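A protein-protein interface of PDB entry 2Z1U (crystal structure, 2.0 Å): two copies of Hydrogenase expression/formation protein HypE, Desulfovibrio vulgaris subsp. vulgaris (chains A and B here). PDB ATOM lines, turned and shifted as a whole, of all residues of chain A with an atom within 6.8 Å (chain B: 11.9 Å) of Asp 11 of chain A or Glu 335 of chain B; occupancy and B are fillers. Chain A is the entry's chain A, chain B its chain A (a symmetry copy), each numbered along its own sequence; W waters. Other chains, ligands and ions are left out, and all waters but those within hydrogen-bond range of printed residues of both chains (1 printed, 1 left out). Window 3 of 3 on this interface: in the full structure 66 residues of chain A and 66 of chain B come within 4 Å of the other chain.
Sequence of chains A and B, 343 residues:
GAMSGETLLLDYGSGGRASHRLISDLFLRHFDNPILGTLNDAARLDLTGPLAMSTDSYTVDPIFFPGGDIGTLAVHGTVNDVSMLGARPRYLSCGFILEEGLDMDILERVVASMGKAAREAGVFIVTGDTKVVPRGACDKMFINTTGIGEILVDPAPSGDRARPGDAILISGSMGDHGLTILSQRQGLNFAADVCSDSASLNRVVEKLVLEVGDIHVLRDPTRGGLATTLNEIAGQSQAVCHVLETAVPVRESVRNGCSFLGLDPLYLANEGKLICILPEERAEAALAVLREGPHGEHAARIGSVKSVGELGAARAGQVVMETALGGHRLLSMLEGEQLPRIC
The guanidinium group of Arg 223 of chain B lies within hydrogen-bond range of the backbone carbonyl oxygen of Gly 13 of chain A (2.8 Å). The backbone NH (N) of Arg 17 of chain A sits at hydrogen-bond distance from the side-chain sulfur (SD) of Met 333 of chain B. OD1 of Asp 11 of chain A lies close to O of Glu 335 of chain B (2.9 Å).
Of the 25 printed residues of chain B, 7 touch a printed residue of chain A. Printed residues of chain B that touch a printed residue of chain A: Arg 223, Gly 224, Thr 228, Met 333, Leu 334, Glu 335 and Gln 338. Among the printed residues, no Asp or Glu carboxylate lies within 4 Å of a Lys or Arg side-chain nitrogen of the other chain.
Among the printed residues, pairs that only touch across the chains: Ser 14 of chain A with Arg 223 of chain B (3.6 Å), Ser 14 of chain A with Leu 334 of chain B (3.6 Å), Gly 15 of chain A with Thr 228 of chain B (3.6 Å), Ser 14 of chain A with Gly 224 of chain B (3.7 Å), Gly 16 of chain A with Met 333 of chain B (3.8 Å) and Ser 14 of chain A with Gln 338 of chain B (3.97 Å).
Water W1 lies within hydrogen-bond range of the backbone carbonyl oxygen (O) of Gly 13 of chain A (2.7 Å), the backbone NH (N) of Val 132 of chain A (2.9 Å) and the guanidinium group (NH2) of Arg 223 of chain B (3.3 Å).
Of chain B, only Glu 335 comes within 4 Å of Asp 11 of chain A. Of chain A, only Asp 11 (2.9 Å) comes within 4 Å of Glu 335 of chain B. No residue of chain B comes within 4 Å of Leu 10 of chain A. Gly 15 of chain A touches just one residue of chain B: Thr 228 (3.6 Å). Gly 16 of chain A touches one residue of chain B. No residue of chain B comes within 4 Å of Ala 18 of chain A. No residue of chain B comes within 4 Å of Ser 19 of chain A. No residue of chain B comes within 4 Å of Val 132 of chain A. Of the printed residues of chain A, Gln 338 of chain B touches Ser 14. Printed residues of chain A within 4 Å of Met 333 of chain B: Gly 16 (3.8 Å) and Arg 17 (3.8 Å). Printed residues of chain A within 4 Å of Arg 223 of chain B: Gly 13 and Ser 14. The nearest residue of chain B that does not touch Asp 11 of chain A is Gln 338 of chain B (5.4 Å). The nearest residue of chain A that does not touch Glu 335 of chain B is Ser 14 of chain A (5.2 Å). The nearest printed residue of chain A that does not touch Gln 338 of chain B is Leu 10 of chain A (4.7 Å).
No position is printed for both chains. Of the 9 pairs that touch across the chains among the printed residues, none has its exchanged pair printed and touching as well.
The backbone NH (N) of Gly 15 of chain A sits at hydrogen-bond distance from the side-chain hydroxyl (OG) of Ser 19 of chain A. The side-chain hydroxyl (OG) of Ser 14 of chain A lies close to the backbone NH (N) of Gly 16 of chain A. The side-chain hydroxyl of Ser 14 of chain A sits at hydrogen-bond distance from the backbone carbonyl oxygen of Asp 11 of chain A, 3.0 Å away.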
ATOM      1  N   LEU A   8     -23.194  31.970  14.753  1.00  0.00           N
ATOM      2  CA  LEU A   8     -23.575  31.962  16.176  1.00  0.00           C
ATOM      3  C   LEU A   8     -24.343  30.681  16.534  1.00  0.00           C
ATOM      4  O   LEU A   8     -25.568  30.598  16.384  1.00  0.00           O
ATOM      5  CB  LEU A   8     -24.344  33.223  16.597  1.00  0.00           C
ATOM      6  CG  LEU A   8     -24.623  33.313  18.105  1.00  0.00           C
ATOM      7  CD1 LEU A   8     -23.469  33.929  18.909  1.00  0.00           C
ATOM      8  CD2 LEU A   8     -25.899  34.074  18.359  1.00  0.00           C
ATOM      9  N   LEU A   9     -23.601  29.682  16.999  1.00  0.00           N
ATOM     10  CA  LEU A   9     -24.179  28.388  17.339  1.00  0.00           C
ATOM     11  C   LEU A   9     -24.954  28.494  18.638  1.00  0.00           C
ATOM     12  O   LEU A   9     -24.662  29.357  19.472  1.00  0.00           O
ATOM     13  CB  LEU A   9     -23.091  27.316  17.480  1.00  0.00           C
ATOM     14  CG  LEU A   9     -22.232  26.844  16.290  1.00  0.00           C
ATOM     15  CD1 LEU A   9     -22.995  26.882  14.969  1.00  0.00           C
ATOM     16  CD2 LEU A   9     -20.964  27.670  16.182  1.00  0.00           C
ATOM     17  N   LEU A  10     -25.941  27.616  18.804  1.00  0.00           N
ATOM     18  CA  LEU A  10     -26.636  27.472  20.082  1.00  0.00           C
ATOM     19  C   LEU A  10     -25.660  27.335  21.246  1.00  0.00           C
ATOM     20  O   LEU A  10     -25.909  27.865  22.319  1.00  0.00           O
ATOM     21  CB  LEU A  10     -27.599  26.287  20.061  1.00  0.00           C
ATOM     22  CG  LEU A  10     -29.061  26.568  19.697  1.00  0.00           C
ATOM     23  CD1 LEU A  10     -29.895  25.306  19.902  1.00  0.00           C
ATOM     24  CD2 LEU A  10     -29.648  27.747  20.509  1.00  0.00           C
ATOM     25  N   ASP A  11     -24.544  26.638  21.011  1.00  0.00           N
ATOM     26  CA  ASP A  11     -23.478  26.436  22.009  1.00  0.00           C
ATOM     27  C   ASP A  11     -23.094  27.684  22.796  1.00  0.00           C
ATOM     28  O   ASP A  11     -22.711  27.582  23.962  1.00  0.00           O
ATOM     29  CB  ASP A  11     -22.200  25.910  21.342  1.00  0.00           C
ATOM     30  CG  ASP A  11     -22.456  24.754  20.392  1.00  0.00           C
ATOM     31  OD1 ASP A  11     -21.628  23.819  20.393  1.00  0.00           O
ATOM     32  OD2 ASP A  11     -23.455  24.784  19.629  1.00  0.00           O
ATOM     33  N   TYR A  12     -23.172  28.851  22.151  1.00  0.00           N
ATOM     34  CA  TYR A  12     -22.790  30.117  22.781  1.00  0.00           C
ATOM     35  C   TYR A  12     -23.776  30.576  23.850  1.00  0.00           C
ATOM     36  O   TYR A  12     -23.477  31.508  24.603  1.00  0.00           O
ATOM     37  CB  TYR A  12     -22.573  31.218  21.734  1.00  0.00           C
ATOM     38  CG  TYR A  12     -21.292  31.049  20.934  1.00  0.00           C
ATOM     39  CD1 TYR A  12     -21.330  30.865  19.551  1.00  0.00           C
ATOM     40  CD2 TYR A  12     -20.043  31.072  21.562  1.00  0.00           C
ATOM     41  CE1 TYR A  12     -20.155  30.705  18.805  1.00  0.00           C
ATOM     42  CE2 TYR A  12     -18.855  30.904  20.819  1.00  0.00           C
ATOM     43  CZ  TYR A  12     -18.927  30.731  19.450  1.00  0.00           C
ATOM     44  OH  TYR A  12     -17.763  30.566  18.724  1.00  0.00           O
ATOM     45  N   GLY A  13     -24.934  29.920  23.924  1.00  0.00           N
ATOM     46  CA  GLY A  13     -25.937  30.227  24.947  1.00  0.00           C
ATOM     47  C   GLY A  13     -26.137  29.161  26.014  1.00  0.00           C
ATOM     48  O   GLY A  13     -27.022  29.292  26.876  1.00  0.00           O
ATOM     49  N   SER A  14     -25.306  28.119  25.968  1.00  0.00           N
ATOM     50  CA  SER A  14     -25.438  26.959  26.858  1.00  0.00           C
ATOM     51  C   SER A  14     -24.806  27.186  28.230  1.00  0.00           C
ATOM     52  O   SER A  14     -25.092  26.454  29.172  1.00  0.00           O
ATOM     53  CB  SER A  14     -24.832  25.712  26.212  1.00  0.00           C
ATOM     54  OG  SER A  14     -23.420  25.755  26.293  1.00  0.00           O
ATOM     55  N   GLY A  15     -23.939  28.193  28.326  1.00  0.00           N
ATOM     56  CA  GLY A  15     -23.260  28.519  29.573  1.00  0.00           C
ATOM     57  C   GLY A  15     -21.949  27.784  29.793  1.00  0.00           C
ATOM     58  O   GLY A  15     -21.378  27.863  30.881  1.00  0.00           O
ATOM     59  N   GLY A  16     -21.470  27.078  28.766  1.00  0.00           N
ATOM     60  CA  GLY A  16     -20.243  26.269  28.832  1.00  0.00           C
ATOM     61  C   GLY A  16     -18.989  26.986  28.354  1.00  0.00           C
ATOM     62  O   GLY A  16     -18.891  28.207  28.464  1.00  0.00           O
ATOM     63  N   ARG A  17     -18.031  26.229  27.818  1.00  0.00           N
ATOM     64  CA  ARG A  17     -16.726  26.779  27.422  1.00  0.00           C
ATOM     65  C   ARG A  17     -16.788  27.847  26.310  1.00  0.00           C
ATOM     66  O   ARG A  17     -16.111  28.876  26.398  1.00  0.00           O
ATOM     67  CB  ARG A  17     -15.725  25.660  27.053  1.00  0.00           C
ATOM     68  CG  ARG A  17     -16.245  24.622  26.051  1.00  0.00           C
ATOM     69  CD  ARG A  17     -15.102  23.835  25.336  1.00  0.00           C
ATOM     70  NE  ARG A  17     -14.336  24.715  24.454  1.00  0.00           N
ATOM     71  CZ  ARG A  17     -14.745  25.143  23.258  1.00  0.00           C
ATOM     72  NH1 ARG A  17     -15.911  24.756  22.748  1.00  0.00           N
ATOM     73  NH2 ARG A  17     -13.973  25.964  22.565  1.00  0.00           N
ATOM     74  N   ALA A  18     -17.582  27.587  25.270  1.00  0.00           N
ATOM     75  CA  ALA A  18     -17.777  28.542  24.171  1.00  0.00           C
ATOM     76  C   ALA A  18     -18.481  29.835  24.652  1.00  0.00           C
ATOM     77  O   ALA A  18     -18.136  30.944  24.211  1.00  0.00           O
ATOM     78  CB  ALA A  18     -18.556  27.897  23.039  1.00  0.00           C
ATOM     79  N   SER A  19     -19.461  29.686  25.540  1.00  0.00           N
ATOM     80  CA  SER A  19     -20.106  30.842  26.176  1.00  0.00           C
ATOM     81  C   SER A  19     -19.071  31.754  26.827  1.00  0.00           C
ATOM     82  O   SER A  19     -19.051  32.959  26.566  1.00  0.00           O
ATOM     83  CB  SER A  19     -21.141  30.408  27.231  1.00  0.00           C
ATOM     84  OG  SER A  19     -22.413  30.164  26.654  1.00  0.00           O
ATOM     85  N   GLU A 100     -29.836  31.915  17.255  1.00  0.00           N
ATOM     86  CA  GLU A 100     -28.987  30.878  16.645  1.00  0.00           C
ATOM     87  C   GLU A 100     -28.880  31.116  15.144  1.00  0.00           C
ATOM     88  O   GLU A 100     -29.874  31.438  14.498  1.00  0.00           O
ATOM     89  CB  GLU A 100     -29.582  29.487  16.919  1.00  0.00           C
ATOM     90  CG  GLU A 100     -28.831  28.313  16.309  1.00  0.00           C
ATOM     91  CD  GLU A 100     -29.666  27.030  16.229  1.00  0.00           C
ATOM     92  OE1 GLU A 100     -29.066  25.945  16.096  1.00  0.00           O
ATOM     93  OE2 GLU A 100     -30.913  27.101  16.292  1.00  0.00           O
ATOM     94  N   VAL A 132     -28.765  32.879  23.929  1.00  0.00           N
ATOM     95  CA  VAL A 132     -28.917  32.512  22.522  1.00  0.00           C
ATOM     96  C   VAL A 132     -30.113  31.574  22.411  1.00  0.00           C
ATOM     97  O   VAL A 132     -30.134  30.513  23.032  1.00  0.00           O
ATOM     98  CB  VAL A 132     -27.644  31.825  21.948  1.00  0.00           C
ATOM     99  CG1 VAL A 132     -27.813  31.535  20.447  1.00  0.00           C
ATOM    100  CG2 VAL A 132     -26.400  32.693  22.178  1.00  0.00           C
ATOM    101  N   ARG B 223     -27.082  27.938  34.295  1.00  0.00           N
ATOM    102  CA  ARG B 223     -26.723  27.266  33.040  1.00  0.00           C
ATOM    103  C   ARG B 223     -25.410  26.550  33.193  1.00  0.00           C
ATOM    104  O   ARG B 223     -24.454  27.113  33.716  1.00  0.00           O
ATOM    105  CB  ARG B 223     -26.642  28.235  31.865  1.00  0.00           C
ATOM    106  CG  ARG B 223     -27.989  28.700  31.395  1.00  0.00           C
ATOM    107  CD  ARG B 223     -27.930  30.219  31.223  1.00  0.00           C
ATOM    108  NE  ARG B 223     -27.501  30.518  29.894  1.00  0.00           N
ATOM    109  CZ  ARG B 223     -26.937  31.649  29.477  1.00  0.00           C
ATOM    110  NH1 ARG B 223     -26.656  32.657  30.290  1.00  0.00           N
ATOM    111  NH2 ARG B 223     -26.617  31.731  28.206  1.00  0.00           N
ATOM    112  N   GLY B 224     -25.371  25.303  32.730  1.00  0.00           N
ATOM    113  CA  GLY B 224     -24.204  24.455  32.914  1.00  0.00           C
ATOM    114  C   GLY B 224     -24.193  23.691  34.229  1.00  0.00           C
ATOM    115  O   GLY B 224     -23.416  22.756  34.384  1.00  0.00           O
ATOM    116  N   GLY B 225     -25.033  24.103  35.184  1.00  0.00           N
ATOM    117  CA  GLY B 225     -25.216  23.346  36.425  1.00  0.00           C
ATOM    118  C   GLY B 225     -24.048  23.436  37.395  1.00  0.00           C
ATOM    119  O   GLY B 225     -23.167  24.288  37.244  1.00  0.00           O
ATOM    120  N   ALA B 227     -21.505  21.466  37.813  1.00  0.00           N
ATOM    121  CA  ALA B 227     -20.196  21.167  37.226  1.00  0.00           C
ATOM    122  C   ALA B 227     -19.588  22.405  36.567  1.00  0.00           C
ATOM    123  O   ALA B 227     -18.435  22.728  36.823  1.00  0.00           O
ATOM    124  CB  ALA B 227     -20.284  20.003  36.269  1.00  0.00           C
ATOM    125  N   THR B 228     -20.351  23.258  35.854  1.00  0.00           N
ATOM    126  CA  THR B 228     -19.627  24.302  35.180  1.00  0.00           C
ATOM    127  C   THR B 228     -19.516  25.565  36.104  1.00  0.00           C
ATOM    128  O   THR B 228     -18.409  26.228  36.018  1.00  0.00           O
ATOM    129  CB  THR B 228     -20.229  24.748  33.833  1.00  0.00           C
ATOM    130  OG1 THR B 228     -20.213  23.648  32.914  1.00  0.00           O
ATOM    131  CG2 THR B 228     -19.427  25.902  33.250  1.00  0.00           C
ATOM    132  N   ASN B 231     -16.203  24.696  37.876  1.00  0.00           N
ATOM    133  CA  ASN B 231     -15.094  24.936  36.934  1.00  0.00           C
ATOM    134  C   ASN B 231     -14.762  26.434  36.851  1.00  0.00           C
ATOM    135  O   ASN B 231     -13.583  26.815  36.782  1.00  0.00           O
ATOM    136  CB  ASN B 231     -15.455  24.426  35.546  1.00  0.00           C
ATOM    137  CG  ASN B 231     -15.082  22.997  35.345  1.00  0.00           C
ATOM    138  OD1 ASN B 231     -15.906  22.101  35.520  1.00  0.00           O
ATOM    139  ND2 ASN B 231     -13.830  22.760  35.007  1.00  0.00           N
ATOM    140  N   GLU B 232     -15.810  27.273  36.865  1.00  0.00           N
ATOM    141  CA  GLU B 232     -15.632  28.728  36.858  1.00  0.00           C
ATOM    142  C   GLU B 232     -14.852  29.154  38.087  1.00  0.00           C
ATOM    143  O   GLU B 232     -13.853  29.860  37.983  1.00  0.00           O
ATOM    144  CB  GLU B 232     -16.976  29.465  36.842  1.00  0.00           C
ATOM    145  CG  GLU B 232     -17.789  29.240  35.599  1.00  0.00           C
ATOM    146  CD  GLU B 232     -19.132  29.945  35.687  1.00  0.00           C
ATOM    147  OE1 GLU B 232     -19.794  30.091  34.645  1.00  0.00           O
ATOM    148  OE2 GLU B 232     -19.493  30.397  36.780  1.00  0.00           O
ATOM    149  N   GLY B 262     -31.418  10.711  29.251  1.00  0.00           N
ATOM    150  CA  GLY B 262     -29.994  10.820  28.916  1.00  0.00           C
ATOM    151  C   GLY B 262     -29.333  12.101  29.399  1.00  0.00           C
ATOM    152  O   GLY B 262     -28.368  12.579  28.792  1.00  0.00           O
ATOM    153  N   LEU B 263     -29.857  12.655  30.491  1.00  0.00           N
ATOM    154  CA  LEU B 263     -29.364  13.901  31.065  1.00  0.00           C
ATOM    155  C   LEU B 263     -28.477  13.662  32.298  1.00  0.00           C
ATOM    156  O   LEU B 263     -28.630  12.676  33.011  1.00  0.00           O
ATOM    157  CB  LEU B 263     -30.546  14.818  31.446  1.00  0.00           C
ATOM    158  CG  LEU B 263     -31.605  15.203  30.397  1.00  0.00           C
ATOM    159  CD1 LEU B 263     -32.802  15.896  31.061  1.00  0.00           C
ATOM    160  CD2 LEU B 263     -31.023  16.076  29.292  1.00  0.00           C
ATOM    161  N   ASP B 264     -27.562  14.593  32.549  1.00  0.00           N
ATOM    162  CA  ASP B 264     -26.674  14.524  33.708  1.00  0.00           C
ATOM    163  C   ASP B 264     -27.098  15.609  34.701  1.00  0.00           C
ATOM    164  O   ASP B 264     -26.997  16.799  34.392  1.00  0.00           O
ATOM    165  CB  ASP B 264     -25.220  14.715  33.241  1.00  0.00           C
ATOM    166  CG  ASP B 264     -24.198  14.469  34.341  1.00  0.00           C
ATOM    167  OD1 ASP B 264     -23.068  14.076  33.985  1.00  0.00           O
ATOM    168  OD2 ASP B 264     -24.504  14.649  35.541  1.00  0.00           O
ATOM    169  N   LEU B 266     -25.755  16.843  37.182  1.00  0.00           N
ATOM    170  CA  LEU B 266     -24.675  17.764  37.570  1.00  0.00           C
ATOM    171  C   LEU B 266     -24.442  18.923  36.597  1.00  0.00           C
ATOM    172  O   LEU B 266     -23.674  19.839  36.900  1.00  0.00           O
ATOM    173  CB  LEU B 266     -23.367  16.998  37.778  1.00  0.00           C
ATOM    174  CG  LEU B 266     -23.382  15.753  38.672  1.00  0.00           C
ATOM    175  CD1 LEU B 266     -22.020  15.062  38.575  1.00  0.00           C
ATOM    176  CD2 LEU B 266     -23.745  16.101  40.115  1.00  0.00           C
ATOM    177  N   TYR B 267     -25.069  18.853  35.425  1.00  0.00           N
ATOM    178  CA  TYR B 267     -24.922  19.873  34.382  1.00  0.00           C
ATOM    179  C   TYR B 267     -26.236  20.573  34.060  1.00  0.00           C
ATOM    180  O   TYR B 267     -26.275  21.439  33.178  1.00  0.00           O
ATOM    181  CB  TYR B 267     -24.347  19.270  33.096  1.00  0.00           C
ATOM    182  CG  TYR B 267     -22.895  18.871  33.197  1.00  0.00           C
ATOM    183  CD1 TYR B 267     -22.526  17.664  33.779  1.00  0.00           C
ATOM    184  CD2 TYR B 267     -21.893  19.724  32.759  1.00  0.00           C
ATOM    185  CE1 TYR B 267     -21.163  17.284  33.888  1.00  0.00           C
ATOM    186  CE2 TYR B 267     -20.537  19.357  32.847  1.00  0.00           C
ATOM    187  CZ  TYR B 267     -20.179  18.148  33.422  1.00  0.00           C
ATOM    188  OH  TYR B 267     -18.837  17.803  33.510  1.00  0.00           O
ATOM    189  N   LEU B 268     -27.306  20.196  34.759  1.00  0.00           N
ATOM    190  CA  LEU B 268     -28.626  20.801  34.537  1.00  0.00           C
ATOM    191  C   LEU B 268     -28.804  22.038  35.392  1.00  0.00           C
ATOM    192  O   LEU B 268     -28.386  22.060  36.553  1.00  0.00           O
ATOM    193  CB  LEU B 268     -29.746  19.806  34.843  1.00  0.00           C
ATOM    194  CG  LEU B 268     -30.050  18.723  33.809  1.00  0.00           C
ATOM    195  CD1 LEU B 268     -31.156  17.822  34.332  1.00  0.00           C
ATOM    196  CD2 LEU B 268     -30.417  19.335  32.438  1.00  0.00           C
ATOM    197  N   ARG B 329     -13.807  10.948  38.319  1.00  0.00           N
ATOM    198  CA  ARG B 329     -14.356  11.515  37.101  1.00  0.00           C
ATOM    199  C   ARG B 329     -14.003  12.991  37.059  1.00  0.00           C
ATOM    200  O   ARG B 329     -14.282  13.749  38.006  1.00  0.00           O
ATOM    201  CB  ARG B 329     -15.880  11.298  37.025  1.00  0.00           C
ATOM    202  CG  ARG B 329     -16.653  12.425  36.361  1.00  0.00           C
ATOM    203  CD  ARG B 329     -17.587  11.942  35.271  1.00  0.00           C
ATOM    204  NE  ARG B 329     -18.881  11.602  35.824  1.00  0.00           N
ATOM    205  CZ  ARG B 329     -20.017  12.278  35.629  1.00  0.00           C
ATOM    206  NH1 ARG B 329     -20.077  13.346  34.832  1.00  0.00           N
ATOM    207  NH2 ARG B 329     -21.111  11.833  36.235  1.00  0.00           N
ATOM    208  N   LEU B 330     -13.389  13.403  35.956  1.00  0.00           N
ATOM    209  CA  LEU B 330     -13.144  14.819  35.702  1.00  0.00           C
ATOM    210  C   LEU B 330     -14.449  15.451  35.231  1.00  0.00           C
ATOM    211  O   LEU B 330     -15.045  14.986  34.262  1.00  0.00           O
ATOM    212  CB  LEU B 330     -12.022  14.972  34.656  1.00  0.00           C
ATOM    213  CG  LEU B 330     -11.550  16.382  34.298  1.00  0.00           C
ATOM    214  CD1 LEU B 330     -10.971  17.133  35.498  1.00  0.00           C
ATOM    215  CD2 LEU B 330     -10.547  16.329  33.139  1.00  0.00           C
ATOM    216  N   LEU B 331     -14.908  16.487  35.937  1.00  0.00           N
ATOM    217  CA  LEU B 331     -16.091  17.237  35.522  1.00  0.00           C
ATOM    218  C   LEU B 331     -15.670  18.457  34.709  1.00  0.00           C
ATOM    219  O   LEU B 331     -15.419  19.518  35.275  1.00  0.00           O
ATOM    220  CB  LEU B 331     -16.925  17.695  36.741  1.00  0.00           C
ATOM    221  CG  LEU B 331     -17.498  16.668  37.731  1.00  0.00           C
ATOM    222  CD1 LEU B 331     -18.364  17.372  38.827  1.00  0.00           C
ATOM    223  CD2 LEU B 331     -18.303  15.608  37.009  1.00  0.00           C
ATOM    224  N   SER B 332     -15.611  18.318  33.390  1.00  0.00           N
ATOM    225  CA  SER B 332     -15.263  19.445  32.520  1.00  0.00           C
ATOM    226  C   SER B 332     -16.509  20.186  32.060  1.00  0.00           C
ATOM    227  O   SER B 332     -17.620  19.700  32.244  1.00  0.00           O
ATOM    228  CB  SER B 332     -14.448  18.964  31.319  1.00  0.00           C
ATOM    229  OG  SER B 332     -13.310  18.246  31.757  1.00  0.00           O
ATOM    230  N   MET B 333     -16.321  21.375  31.485  1.00  0.00           N
ATOM    231  CA  MET B 333     -17.387  22.168  30.896  1.00  0.00           C
ATOM    232  C   MET B 333     -17.958  21.494  29.628  1.00  0.00           C
ATOM    233  O   MET B 333     -17.239  20.804  28.885  1.00  0.00           O
ATOM    234  CB  MET B 333     -16.988  23.590  30.595  1.00  0.00           C
ATOM    235  CG  MET B 333     -16.924  24.534  31.803  1.00  0.00           C
ATOM    236  SD  MET B 333     -16.686  26.278  31.322  1.00  0.00           S
ATOM    237  CE  MET B 333     -16.157  26.992  32.874  1.00  0.00           C
ATOM    238  N   LEU B 334     -19.286  21.763  29.378  1.00  0.00           N
ATOM    239  CA  LEU B 334     -20.221  21.150  28.365  1.00  0.00           C
ATOM    240  C   LEU B 334     -19.596  20.999  26.983  1.00  0.00           C
ATOM    241  O   LEU B 334     -18.464  20.624  26.675  1.00  0.00           O
ATOM    242  CB  LEU B 334     -21.459  22.047  28.280  1.00  0.00           C
ATOM    243  CG  LEU B 334     -22.268  22.211  29.569  1.00  0.00           C
ATOM    244  CD1 LEU B 334     -23.305  23.310  29.394  1.00  0.00           C
ATOM    245  CD2 LEU B 334     -22.935  20.895  29.934  1.00  0.00           C
ATOM    246  N   GLU B 335     -20.523  21.181  25.984  1.00  0.00           N
ATOM    247  CA  GLU B 335     -20.350  20.897  24.536  1.00  0.00           C
ATOM    248  C   GLU B 335     -21.257  21.781  23.682  1.00  0.00           C
ATOM    249  O   GLU B 335     -21.189  21.754  22.447  1.00  0.00           O
ATOM    250  CB  GLU B 335     -20.662  19.422  24.261  1.00  0.00           C
ATOM    251  CG  GLU B 335     -19.533  18.459  24.616  1.00  0.00           C
ATOM    252  CD  GLU B 335     -19.996  17.291  25.475  1.00  0.00           C
ATOM    253  OE1 GLU B 335     -19.314  16.236  25.463  1.00  0.00           O
ATOM    254  OE2 GLU B 335     -21.033  17.434  26.171  1.00  0.00           O
ATOM    255  N   GLN B 338     -27.276  22.307  22.626  1.00  0.00           N
ATOM    256  CA  GLN B 338     -27.299  21.593  23.903  1.00  0.00           C
ATOM    257  C   GLN B 338     -28.718  21.478  24.491  1.00  0.00           C
ATOM    258  O   GLN B 338     -29.533  20.659  24.035  1.00  0.00           O
ATOM    259  CB  GLN B 338     -26.373  22.280  24.931  1.00  0.00           C
ATOM    260  CG  GLN B 338     -24.913  21.849  24.887  1.00  0.00           C
ATOM    261  CD  GLN B 338     -24.708  20.441  25.417  1.00  0.00           C
ATOM    262  OE1 GLN B 338     -25.104  20.124  26.543  1.00  0.00           O
ATOM    263  NE2 GLN B 338     -24.084  19.582  24.602  1.00  0.00           N
ATOM    264  N   LEU B 339     -28.984  22.306  25.506  1.00  0.00           N
ATOM    265  CA  LEU B 339     -30.251  22.310  26.247  1.00  0.00           C
ATOM    266  C   LEU B 339     -30.835  23.723  26.223  1.00  0.00           C
ATOM    267  O   LEU B 339     -30.605  24.503  27.148  1.00  0.00           O
ATOM    268  CB  LEU B 339     -30.024  21.858  27.701  1.00  0.00           C
ATOM    269  CG  LEU B 339     -29.180  20.593  27.957  1.00  0.00           C
ATOM    270  CD1 LEU B 339     -28.694  20.538  29.402  1.00  0.00           C
ATOM    271  CD2 LEU B 339     -29.938  19.311  27.585  1.00  0.00           C
ATOM    272  N   PRO B 340     -31.605  24.054  25.169  1.00  0.00           N
ATOM    273  CA  PRO B 340     -31.945  25.460  24.935  1.00  0.00           C
ATOM    274  C   PRO B 340     -33.095  25.951  25.807  1.00  0.00           C
ATOM    275  O   PRO B 340     -33.980  25.168  26.188  1.00  0.00           O
ATOM    276  CB  PRO B 340     -32.345  25.489  23.451  1.00  0.00           C
ATOM    277  CG  PRO B 340     -32.821  24.109  23.153  1.00  0.00           C
ATOM    278  CD  PRO B 340     -32.211  23.161  24.162  1.00  0.00           C
ATOM    279  N   ARG B 341     -33.045  27.236  26.144  1.00  0.00           N
ATOM    280  CA  ARG B 341     -34.153  27.913  26.799  1.00  0.00           C
ATOM    281  C   ARG B 341     -34.639  27.201  28.076  1.00  0.00           C
ATOM    282  O   ARG B 341     -35.840  27.127  28.348  1.00  0.00           O
ATOM    283  CB  ARG B 341     -35.277  28.126  25.778  1.00  0.00           C
ATOM    284  CG  ARG B 341     -34.888  29.131  24.701  1.00  0.00           C
ATOM    285  CD  ARG B 341     -36.012  29.350  23.719  1.00  0.00           C
ATOM    286  NE  ARG B 341     -37.121  30.079  24.318  1.00  0.00           N
ATOM    287  CZ  ARG B 341     -38.304  30.246  23.743  1.00  0.00           C
ATOM    288  NH1 ARG B 341     -38.551  29.720  22.539  1.00  0.00           N
ATOM    289  NH2 ARG B 341     -39.243  30.930  24.376  1.00  0.00           N
ATOM    290  N   ILE B 342     -33.688  26.689  28.856  1.00  0.00           N
ATOM    291  CA  ILE B 342     -34.005  26.092  30.160  1.00  0.00           C
ATOM    292  C   ILE B 342     -34.239  27.172  31.225  1.00  0.00           C
ATOM    293  O   ILE B 342     -34.726  26.886  32.307  1.00  0.00           O
ATOM    294  CB  ILE B 342     -32.938  25.043  30.648  1.00  0.00           C
ATOM    295  CG1 ILE B 342     -31.513  25.529  30.393  1.00  0.00           C
ATOM    296  CG2 ILE B 342     -33.123  23.682  29.928  1.00  0.00           C
ATOM    297  CD1 ILE B 342     -31.029  26.629  31.330  1.00  0.00           C
HETATM  298  O   HOH W   1     -29.035  30.928  26.122  1.00  0.00           O
